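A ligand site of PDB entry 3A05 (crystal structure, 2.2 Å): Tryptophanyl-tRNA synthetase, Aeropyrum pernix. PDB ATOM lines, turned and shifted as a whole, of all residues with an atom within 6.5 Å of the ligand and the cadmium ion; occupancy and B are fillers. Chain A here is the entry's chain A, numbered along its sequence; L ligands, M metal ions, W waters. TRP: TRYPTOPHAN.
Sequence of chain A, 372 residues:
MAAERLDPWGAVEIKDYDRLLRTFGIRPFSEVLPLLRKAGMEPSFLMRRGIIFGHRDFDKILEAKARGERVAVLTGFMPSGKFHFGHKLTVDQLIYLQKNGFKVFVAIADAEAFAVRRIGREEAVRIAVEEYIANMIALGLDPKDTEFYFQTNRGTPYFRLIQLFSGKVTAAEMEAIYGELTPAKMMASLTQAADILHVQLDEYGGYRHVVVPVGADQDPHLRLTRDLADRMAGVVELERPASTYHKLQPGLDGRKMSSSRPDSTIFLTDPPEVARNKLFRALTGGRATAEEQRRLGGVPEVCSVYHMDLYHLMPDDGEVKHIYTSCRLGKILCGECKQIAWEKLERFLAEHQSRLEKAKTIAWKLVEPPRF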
ATOM      1  N   LEU A  74      30.891  31.769 -15.863  1.00  0.00           N
ATOM      2  CA  LEU A  74      30.643  30.366 -15.604  1.00  0.00           C
ATOM      3  C   LEU A  74      29.262  30.045 -16.152  1.00  0.00           C
ATOM      4  O   LEU A  74      28.379  30.909 -16.058  1.00  0.00           O
ATOM      5  CB  LEU A  74      30.669  30.077 -14.065  1.00  0.00           C
ATOM      6  CG  LEU A  74      30.490  28.571 -13.755  1.00  0.00           C
ATOM      7  CD1 LEU A  74      31.423  28.001 -12.745  1.00  0.00           C
ATOM      8  CD2 LEU A  74      29.040  28.312 -13.381  1.00  0.00           C
ATOM      9  N   THR A  75      29.081  28.847 -16.752  1.00  0.00           N
ATOM     10  CA  THR A  75      27.728  28.384 -17.057  1.00  0.00           C
ATOM     11  C   THR A  75      27.833  26.853 -16.979  1.00  0.00           C
ATOM     12  O   THR A  75      28.930  26.299 -16.821  1.00  0.00           O
ATOM     13  CB  THR A  75      27.242  28.856 -18.499  1.00  0.00           C
ATOM     14  OG1 THR A  75      25.890  28.398 -18.711  1.00  0.00           O
ATOM     15  CG2 THR A  75      28.107  28.215 -19.583  1.00  0.00           C
ATOM     16  N   GLY A  76      26.738  26.111 -17.055  1.00  0.00           N
ATOM     17  CA  GLY A  76      26.956  24.690 -17.199  1.00  0.00           C
ATOM     18  C   GLY A  76      26.040  24.118 -18.277  1.00  0.00           C
ATOM     19  O   GLY A  76      25.060  24.787 -18.711  1.00  0.00           O
ATOM     20  N   PHE A  77      26.295  22.853 -18.636  1.00  0.00           N
ATOM     21  CA  PHE A  77      25.447  22.185 -19.676  1.00  0.00           C
ATOM     22  C   PHE A  77      25.013  20.807 -19.209  1.00  0.00           C
ATOM     23  O   PHE A  77      25.808  20.054 -18.653  1.00  0.00           O
ATOM     24  CB  PHE A  77      26.240  22.006 -20.980  1.00  0.00           C
ATOM     25  CG  PHE A  77      26.636  23.285 -21.624  1.00  0.00           C
ATOM     26  CD1 PHE A  77      27.789  23.941 -21.250  1.00  0.00           C
ATOM     27  CD2 PHE A  77      25.784  23.889 -22.570  1.00  0.00           C
ATOM     28  CE1 PHE A  77      28.131  25.156 -21.795  1.00  0.00           C
ATOM     29  CE2 PHE A  77      26.124  25.145 -23.158  1.00  0.00           C
ATOM     30  CZ  PHE A  77      27.294  25.768 -22.788  1.00  0.00           C
ATOM     31  N   MET A  78      23.742  20.499 -19.432  1.00  0.00           N
ATOM     32  CA  MET A  78      23.157  19.176 -19.346  1.00  0.00           C
ATOM     33  C   MET A  78      23.681  18.264 -20.487  1.00  0.00           C
ATOM     34  O   MET A  78      23.356  18.567 -21.654  1.00  0.00           O
ATOM     35  CB  MET A  78      21.627  19.337 -19.494  1.00  0.00           C
ATOM     36  CG  MET A  78      20.827  18.017 -19.432  1.00  0.00           C
ATOM     37  SD  MET A  78      21.330  16.973 -17.993  1.00  0.00           S
ATOM     38  CE  MET A  78      20.659  18.011 -16.720  1.00  0.00           C
ATOM     39  N   ALA A 107      30.650  24.034 -16.441  1.00  0.00           N
ATOM     40  CA  ALA A 107      30.290  22.837 -15.720  1.00  0.00           C
ATOM     41  C   ALA A 107      29.522  21.839 -16.628  1.00  0.00           C
ATOM     42  O   ALA A 107      28.626  22.221 -17.373  1.00  0.00           O
ATOM     43  CB  ALA A 107      29.408  23.158 -14.484  1.00  0.00           C
ATOM     44  N   ILE A 108      29.893  20.557 -16.508  1.00  0.00           N
ATOM     45  CA  ILE A 108      29.087  19.495 -17.017  1.00  0.00           C
ATOM     46  C   ILE A 108      28.211  18.913 -15.923  1.00  0.00           C
ATOM     47  O   ILE A 108      28.720  18.359 -14.922  1.00  0.00           O
ATOM     48  CB  ILE A 108      29.952  18.350 -17.598  1.00  0.00           C
ATOM     49  CG1 ILE A 108      30.946  18.915 -18.620  1.00  0.00           C
ATOM     50  CG2 ILE A 108      29.043  17.251 -18.177  1.00  0.00           C
ATOM     51  CD1 ILE A 108      30.288  19.660 -19.893  1.00  0.00           C
ATOM     52  N   ALA A 109      26.910  19.011 -16.147  1.00  0.00           N
ATOM     53  CA  ALA A 109      25.922  18.590 -15.165  1.00  0.00           C
ATOM     54  C   ALA A 109      25.610  17.164 -15.183  1.00  0.00           C
ATOM     55  O   ALA A 109      24.461  16.833 -15.207  1.00  0.00           O
ATOM     56  CB  ALA A 109      24.624  19.405 -15.313  1.00  0.00           C
ATOM     57  N   GLU A 112      23.341  15.834 -12.219  1.00  0.00           N
ATOM     58  CA  GLU A 112      21.919  16.069 -12.527  1.00  0.00           C
ATOM     59  C   GLU A 112      21.404  15.160 -13.672  1.00  0.00           C
ATOM     60  O   GLU A 112      20.282  14.655 -13.610  1.00  0.00           O
ATOM     61  CB  GLU A 112      21.692  17.504 -12.897  1.00  0.00           C
ATOM     62  CG  GLU A 112      20.210  17.820 -12.999  1.00  0.00           C
ATOM     63  CD  GLU A 112      19.976  19.229 -13.498  1.00  0.00           C
ATOM     64  OE1 GLU A 112      20.950  20.042 -13.560  1.00  0.00           O
ATOM     65  OE2 GLU A 112      18.804  19.523 -13.782  1.00  0.00           O
ATOM     66  N   ARG A 117      17.614  13.167 -14.741  1.00  0.00           N
ATOM     67  CA  ARG A 117      17.180  12.751 -16.116  1.00  0.00           C
ATOM     68  C   ARG A 117      17.390  11.293 -16.395  1.00  0.00           C
ATOM     69  O   ARG A 117      17.106  10.852 -17.501  1.00  0.00           O
ATOM     70  CB  ARG A 117      17.926  13.493 -17.215  1.00  0.00           C
ATOM     71  CG  ARG A 117      17.913  14.992 -17.172  1.00  0.00           C
ATOM     72  CD  ARG A 117      16.596  15.596 -17.521  1.00  0.00           C
ATOM     73  NE  ARG A 117      16.722  17.052 -17.643  1.00  0.00           N
ATOM     74  CZ  ARG A 117      17.014  17.712 -18.773  1.00  0.00           C
ATOM     75  NH1 ARG A 117      17.234  17.051 -19.919  1.00  0.00           N
ATOM     76  NH2 ARG A 117      17.059  19.041 -18.733  1.00  0.00           N
ATOM     77  N   TYR A 149      34.657  20.891 -16.135  1.00  0.00           N
ATOM     78  CA  TYR A 149      34.683  19.949 -15.035  1.00  0.00           C
ATOM     79  C   TYR A 149      33.375  19.269 -14.994  1.00  0.00           C
ATOM     80  O   TYR A 149      32.377  19.797 -15.492  1.00  0.00           O
ATOM     81  CB  TYR A 149      35.008  20.650 -13.660  1.00  0.00           C
ATOM     82  CG  TYR A 149      33.874  21.540 -13.141  1.00  0.00           C
ATOM     83  CD1 TYR A 149      32.824  20.992 -12.439  1.00  0.00           C
ATOM     84  CD2 TYR A 149      33.897  22.929 -13.334  1.00  0.00           C
ATOM     85  CE1 TYR A 149      31.813  21.806 -11.947  1.00  0.00           C
ATOM     86  CE2 TYR A 149      32.849  23.762 -12.821  1.00  0.00           C
ATOM     87  CZ  TYR A 149      31.868  23.191 -12.113  1.00  0.00           C
ATOM     88  OH  TYR A 149      30.788  23.875 -11.691  1.00  0.00           O
ATOM     89  N   GLN A 151      30.389  17.718 -12.488  1.00  0.00           N
ATOM     90  CA  GLN A 151      29.767  17.882 -11.172  1.00  0.00           C
ATOM     91  C   GLN A 151      30.253  16.747 -10.250  1.00  0.00           C
ATOM     92  O   GLN A 151      30.530  16.962  -9.060  1.00  0.00           O
ATOM     93  CB  GLN A 151      28.260  17.841 -11.257  1.00  0.00           C
ATOM     94  CG  GLN A 151      27.665  19.176 -11.779  1.00  0.00           C
ATOM     95  CD  GLN A 151      26.147  19.162 -11.880  1.00  0.00           C
ATOM     96  OE1 GLN A 151      25.551  18.120 -11.985  1.00  0.00           O
ATOM     97  NE2 GLN A 151      25.547  20.317 -11.893  1.00  0.00           N
ATOM     98  N   TYR A 178      10.869  24.987  -8.420  1.00  0.00           N
ATOM     99  CA  TYR A 178      10.947  23.707  -9.086  1.00  0.00           C
ATOM    100  C   TYR A 178       9.606  22.979  -9.111  1.00  0.00           C
ATOM    101  O   TYR A 178       9.402  22.092  -9.939  1.00  0.00           O
ATOM    102  CB  TYR A 178      11.965  22.836  -8.361  1.00  0.00           C
ATOM    103  CG  TYR A 178      13.372  22.925  -8.903  1.00  0.00           C
ATOM    104  CD1 TYR A 178      14.196  24.010  -8.611  1.00  0.00           C
ATOM    105  CD2 TYR A 178      13.898  21.901  -9.700  1.00  0.00           C
ATOM    106  CE1 TYR A 178      15.506  24.093  -9.117  1.00  0.00           C
ATOM    107  CE2 TYR A 178      15.207  21.946 -10.195  1.00  0.00           C
ATOM    108  CZ  TYR A 178      16.001  23.052  -9.905  1.00  0.00           C
ATOM    109  OH  TYR A 178      17.299  23.104 -10.411  1.00  0.00           O
ATOM    110  N   ALA A 188      20.055  18.676  -7.189  1.00  0.00           N
ATOM    111  CA  ALA A 188      20.467  19.444  -8.396  1.00  0.00           C
ATOM    112  C   ALA A 188      20.533  20.960  -8.128  1.00  0.00           C
ATOM    113  O   ALA A 188      21.416  21.694  -8.564  1.00  0.00           O
ATOM    114  CB  ALA A 188      19.510  19.104  -9.541  1.00  0.00           C
ATOM    115  N   SER A 189      19.526  21.448  -7.464  1.00  0.00           N
ATOM    116  CA  SER A 189      19.449  22.843  -7.133  1.00  0.00           C
ATOM    117  C   SER A 189      20.655  23.319  -6.278  1.00  0.00           C
ATOM    118  O   SER A 189      21.279  24.323  -6.606  1.00  0.00           O
ATOM    119  CB  SER A 189      18.118  23.091  -6.411  1.00  0.00           C
ATOM    120  OG  SER A 189      17.950  24.473  -6.326  1.00  0.00           O
ATOM    121  N   THR A 191      23.601  21.837  -6.028  1.00  0.00           N
ATOM    122  CA  THR A 191      24.867  21.602  -6.787  1.00  0.00           C
ATOM    123  C   THR A 191      25.078  22.726  -7.791  1.00  0.00           C
ATOM    124  O   THR A 191      26.202  23.185  -8.060  1.00  0.00           O
ATOM    125  CB  THR A 191      24.745  20.187  -7.524  1.00  0.00           C
ATOM    126  OG1 THR A 191      24.564  19.204  -6.530  1.00  0.00           O
ATOM    127  CG2 THR A 191      26.027  19.804  -8.400  1.00  0.00           C
ATOM    128  N   GLN A 192      23.984  23.174  -8.369  1.00  0.00           N
ATOM    129  CA  GLN A 192      24.086  24.264  -9.328  1.00  0.00           C
ATOM    130  C   GLN A 192      24.487  25.551  -8.636  1.00  0.00           C
ATOM    131  O   GLN A 192      25.229  26.323  -9.179  1.00  0.00           O
ATOM    132  CB  GLN A 192      22.771  24.462 -10.090  1.00  0.00           C
ATOM    133  CG  GLN A 192      22.830  25.683 -11.069  1.00  0.00           C
ATOM    134  CD  GLN A 192      21.611  25.773 -12.055  1.00  0.00           C
ATOM    135  OE1 GLN A 192      20.854  24.826 -12.216  1.00  0.00           O
ATOM    136  NE2 GLN A 192      21.477  26.893 -12.718  1.00  0.00           N
ATOM    137  N   ALA A 193      24.031  25.776  -7.412  1.00  0.00           N
ATOM    138  CA  ALA A 193      24.477  26.973  -6.701  1.00  0.00           C
ATOM    139  C   ALA A 193      25.947  26.783  -6.444  1.00  0.00           C
ATOM    140  O   ALA A 193      26.724  27.724  -6.452  1.00  0.00           O
ATOM    141  CB  ALA A 193      23.694  27.111  -5.283  1.00  0.00           C
ATOM    142  N   ASP A 195      28.008  25.067  -8.256  1.00  0.00           N
ATOM    143  CA  ASP A 195      28.785  25.291  -9.532  1.00  0.00           C
ATOM    144  C   ASP A 195      29.109  26.778  -9.627  1.00  0.00           C
ATOM    145  O   ASP A 195      30.235  27.167  -9.919  1.00  0.00           O
ATOM    146  CB  ASP A 195      27.927  24.905 -10.752  1.00  0.00           C
ATOM    147  CG  ASP A 195      27.757  23.427 -10.901  1.00  0.00           C
ATOM    148  OD1 ASP A 195      28.712  22.675 -10.618  1.00  0.00           O
ATOM    149  OD2 ASP A 195      26.659  23.002 -11.293  1.00  0.00           O
ATOM    150  N   ILE A 196      28.117  27.617  -9.416  1.00  0.00           N
ATOM    151  CA  ILE A 196      28.313  29.069  -9.546  1.00  0.00           C
ATOM    152  C   ILE A 196      29.249  29.692  -8.506  1.00  0.00           C
ATOM    153  O   ILE A 196      30.164  30.485  -8.795  1.00  0.00           O
ATOM    154  CB  ILE A 196      26.948  29.729  -9.475  1.00  0.00           C
ATOM    155  CG1 ILE A 196      26.167  29.352 -10.729  1.00  0.00           C
ATOM    156  CG2 ILE A 196      27.069  31.245  -9.424  1.00  0.00           C
ATOM    157  CD1 ILE A 196      24.586  29.647 -10.624  1.00  0.00           C
ATOM    158  N   VAL A 212      27.149  35.018 -14.739  1.00  0.00           N
ATOM    159  CA  VAL A 212      26.461  33.873 -15.305  1.00  0.00           C
ATOM    160  C   VAL A 212      25.483  34.370 -16.394  1.00  0.00           C
ATOM    161  O   VAL A 212      24.616  35.168 -16.126  1.00  0.00           O
ATOM    162  CB  VAL A 212      25.644  33.095 -14.270  1.00  0.00           C
ATOM    163  CG1 VAL A 212      25.039  31.769 -14.871  1.00  0.00           C
ATOM    164  CG2 VAL A 212      26.534  32.755 -13.003  1.00  0.00           C
ATOM    165  N   PRO A 213      25.687  33.928 -17.650  1.00  0.00           N
ATOM    166  CA  PRO A 213      24.834  34.373 -18.762  1.00  0.00           C
ATOM    167  C   PRO A 213      23.652  33.434 -18.846  1.00  0.00           C
ATOM    168  O   PRO A 213      23.849  32.234 -19.058  1.00  0.00           O
ATOM    169  CB  PRO A 213      25.754  34.238 -19.960  1.00  0.00           C
ATOM    170  CG  PRO A 213      26.642  33.083 -19.642  1.00  0.00           C
ATOM    171  CD  PRO A 213      26.855  33.128 -18.105  1.00  0.00           C
ATOM    172  N   VAL A 214      22.439  33.951 -18.674  1.00  0.00           N
ATOM    173  CA  VAL A 214      21.260  33.128 -18.643  1.00  0.00           C
ATOM    174  C   VAL A 214      20.081  33.781 -19.391  1.00  0.00           C
ATOM    175  O   VAL A 214      20.186  34.928 -19.843  1.00  0.00           O
ATOM    176  CB  VAL A 214      20.725  32.982 -17.160  1.00  0.00           C
ATOM    177  CG1 VAL A 214      21.759  32.343 -16.271  1.00  0.00           C
ATOM    178  CG2 VAL A 214      20.295  34.335 -16.623  1.00  0.00           C
ATOM    179  N   GLN A 218      15.586  31.719 -16.078  1.00  0.00           N
ATOM    180  CA  GLN A 218      16.498  31.039 -15.171  1.00  0.00           C
ATOM    181  C   GLN A 218      16.819  31.890 -13.931  1.00  0.00           C
ATOM    182  O   GLN A 218      17.610  31.454 -13.095  1.00  0.00           O
ATOM    183  CB  GLN A 218      17.825  30.704 -15.869  1.00  0.00           C
ATOM    184  CG  GLN A 218      17.834  29.649 -17.005  1.00  0.00           C
ATOM    185  CD  GLN A 218      19.167  29.681 -17.803  1.00  0.00           C
ATOM    186  OE1 GLN A 218      19.244  30.255 -18.900  1.00  0.00           O
ATOM    187  NE2 GLN A 218      20.262  29.093 -17.207  1.00  0.00           N
ATOM    188  N   LEU A 222      19.047  31.694  -9.845  1.00  0.00           N
ATOM    189  CA  LEU A 222      20.160  32.609  -9.557  1.00  0.00           C
ATOM    190  C   LEU A 222      19.911  33.423  -8.240  1.00  0.00           C
ATOM    191  O   LEU A 222      20.825  33.701  -7.510  1.00  0.00           O
ATOM    192  CB  LEU A 222      20.314  33.595 -10.694  1.00  0.00           C
ATOM    193  CG  LEU A 222      21.692  33.801 -11.306  1.00  0.00           C
ATOM    194  CD1 LEU A 222      22.291  32.476 -11.717  1.00  0.00           C
ATOM    195  CD2 LEU A 222      21.448  34.645 -12.568  1.00  0.00           C
HETATM  196  N   TRP L   1      21.020  23.135 -14.454  1.00  0.00           N
HETATM  197  CA  TRP L   1      21.424  23.408 -15.839  1.00  0.00           C
HETATM  198  C   TRP L   1      20.494  22.661 -16.835  1.00  0.00           C
HETATM  199  O   TRP L   1      20.500  22.956 -18.014  1.00  0.00           O
HETATM  200  CB  TRP L   1      22.898  23.040 -16.035  1.00  0.00           C
HETATM  201  CG  TRP L   1      23.806  23.756 -15.038  1.00  0.00           C
HETATM  202  CD1 TRP L   1      24.472  23.173 -13.967  1.00  0.00           C
HETATM  203  CD2 TRP L   1      24.084  25.188 -14.964  1.00  0.00           C
HETATM  204  NE1 TRP L   1      25.209  24.148 -13.299  1.00  0.00           N
HETATM  205  CE2 TRP L   1      24.983  25.379 -13.875  1.00  0.00           C
HETATM  206  CE3 TRP L   1      23.716  26.316 -15.744  1.00  0.00           C
HETATM  207  CZ2 TRP L   1      25.485  26.652 -13.517  1.00  0.00           C
HETATM  208  CZ3 TRP L   1      24.246  27.594 -15.402  1.00  0.00           C
HETATM  209  CH2 TRP L   1      25.114  27.732 -14.283  1.00  0.00           C
HETATM  210 CD    CD M   1      19.210  21.960 -13.885  1.00  0.00          CD
HETATM  211  O   HOH W   1      24.237  29.981 -17.724  1.00  0.00           O
HETATM  212  O   HOH W   2      19.302  22.577 -11.243  1.00  0.00           O
HETATM  213  O   HOH W   3      19.127  21.819 -20.036  1.00  0.00           O
HETATM  214  O   HOH W   4      16.428  22.651 -14.037  1.00  0.00           O
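The side-chain carboxylate (OD2) of Asp 195 sits at hydrogen-bond distance from a nitrogen (NE1) of the ligand (2.7 Å).
N of the ligand sits close to OE1 of Gln 192 (2.8 Å).
Merely in contact with the cadmium ion: Gln 192 (3.7 Å).
Within 4 Å of the cadmium ion: Glu 112 and Gln 192.
CD2 of Leu 74 touches CZ2 of the ligand (3.9 Å).
Thr 75 touches the ligand (OG1 to CZ3, 3.8 Å).
Gly 76 touches the ligand.
Gln 151 touches the ligand (NE2 to CD1, 3.7 Å).
Ile 196 touches the ligand (CG1 to CZ2, 3.9 Å).
Eight residues have an atom within 4 Å of the ligand: Leu 74, Thr 75, Gly 76, Glu 112, Gln 151, Gln 192, Asp 195 and Ile 196.
The nearest printed residue that does not touch the ligand is Ala 109 (4.004 Å).
OD2 of Asp 195 lies within hydrogen-bond range of NE2 of Gln 151, at 3.0 Å.
The backbone carbonyl oxygen of Thr 75 lies within hydrogen-bond range of the backbone NH of Ala 107 (2.9 Å).
O of Glu 112 sits at hydrogen-bond distance from N of Arg 117 (3.3 Å).
The backbone NH of Gln 151 lies within hydrogen-bond range of the backbone carbonyl oxygen of Ile 108.
The backbone NH (N) of Glu 112 sits at hydrogen-bond distance from the side-chain amide oxygen (OE1) of Gln 151.
The side-chain hydroxyl (OH) of Tyr 149 sits at hydrogen-bond distance from the side-chain carboxylate (OD1) of Asp 195, at 2.6 Å.
Water W1 bridges the side-chain hydroxyl (OG1) of Thr 75 (2.5 Å) and the backbone carbonyl oxygen (O) of Pro 213 (2.6 Å).
The cadmium ion is bound by a nitrogen (N) of the ligand (2.2 Å) and the side-chain carboxylate of Glu 112 (2.5 Å).
Slightly farther from the cadmium ion lies the side-chain carboxylate (OE1) of Glu 112 (2.6 Å).
Slightly farther from the cadmium ion lies water W2 (2.7 Å).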
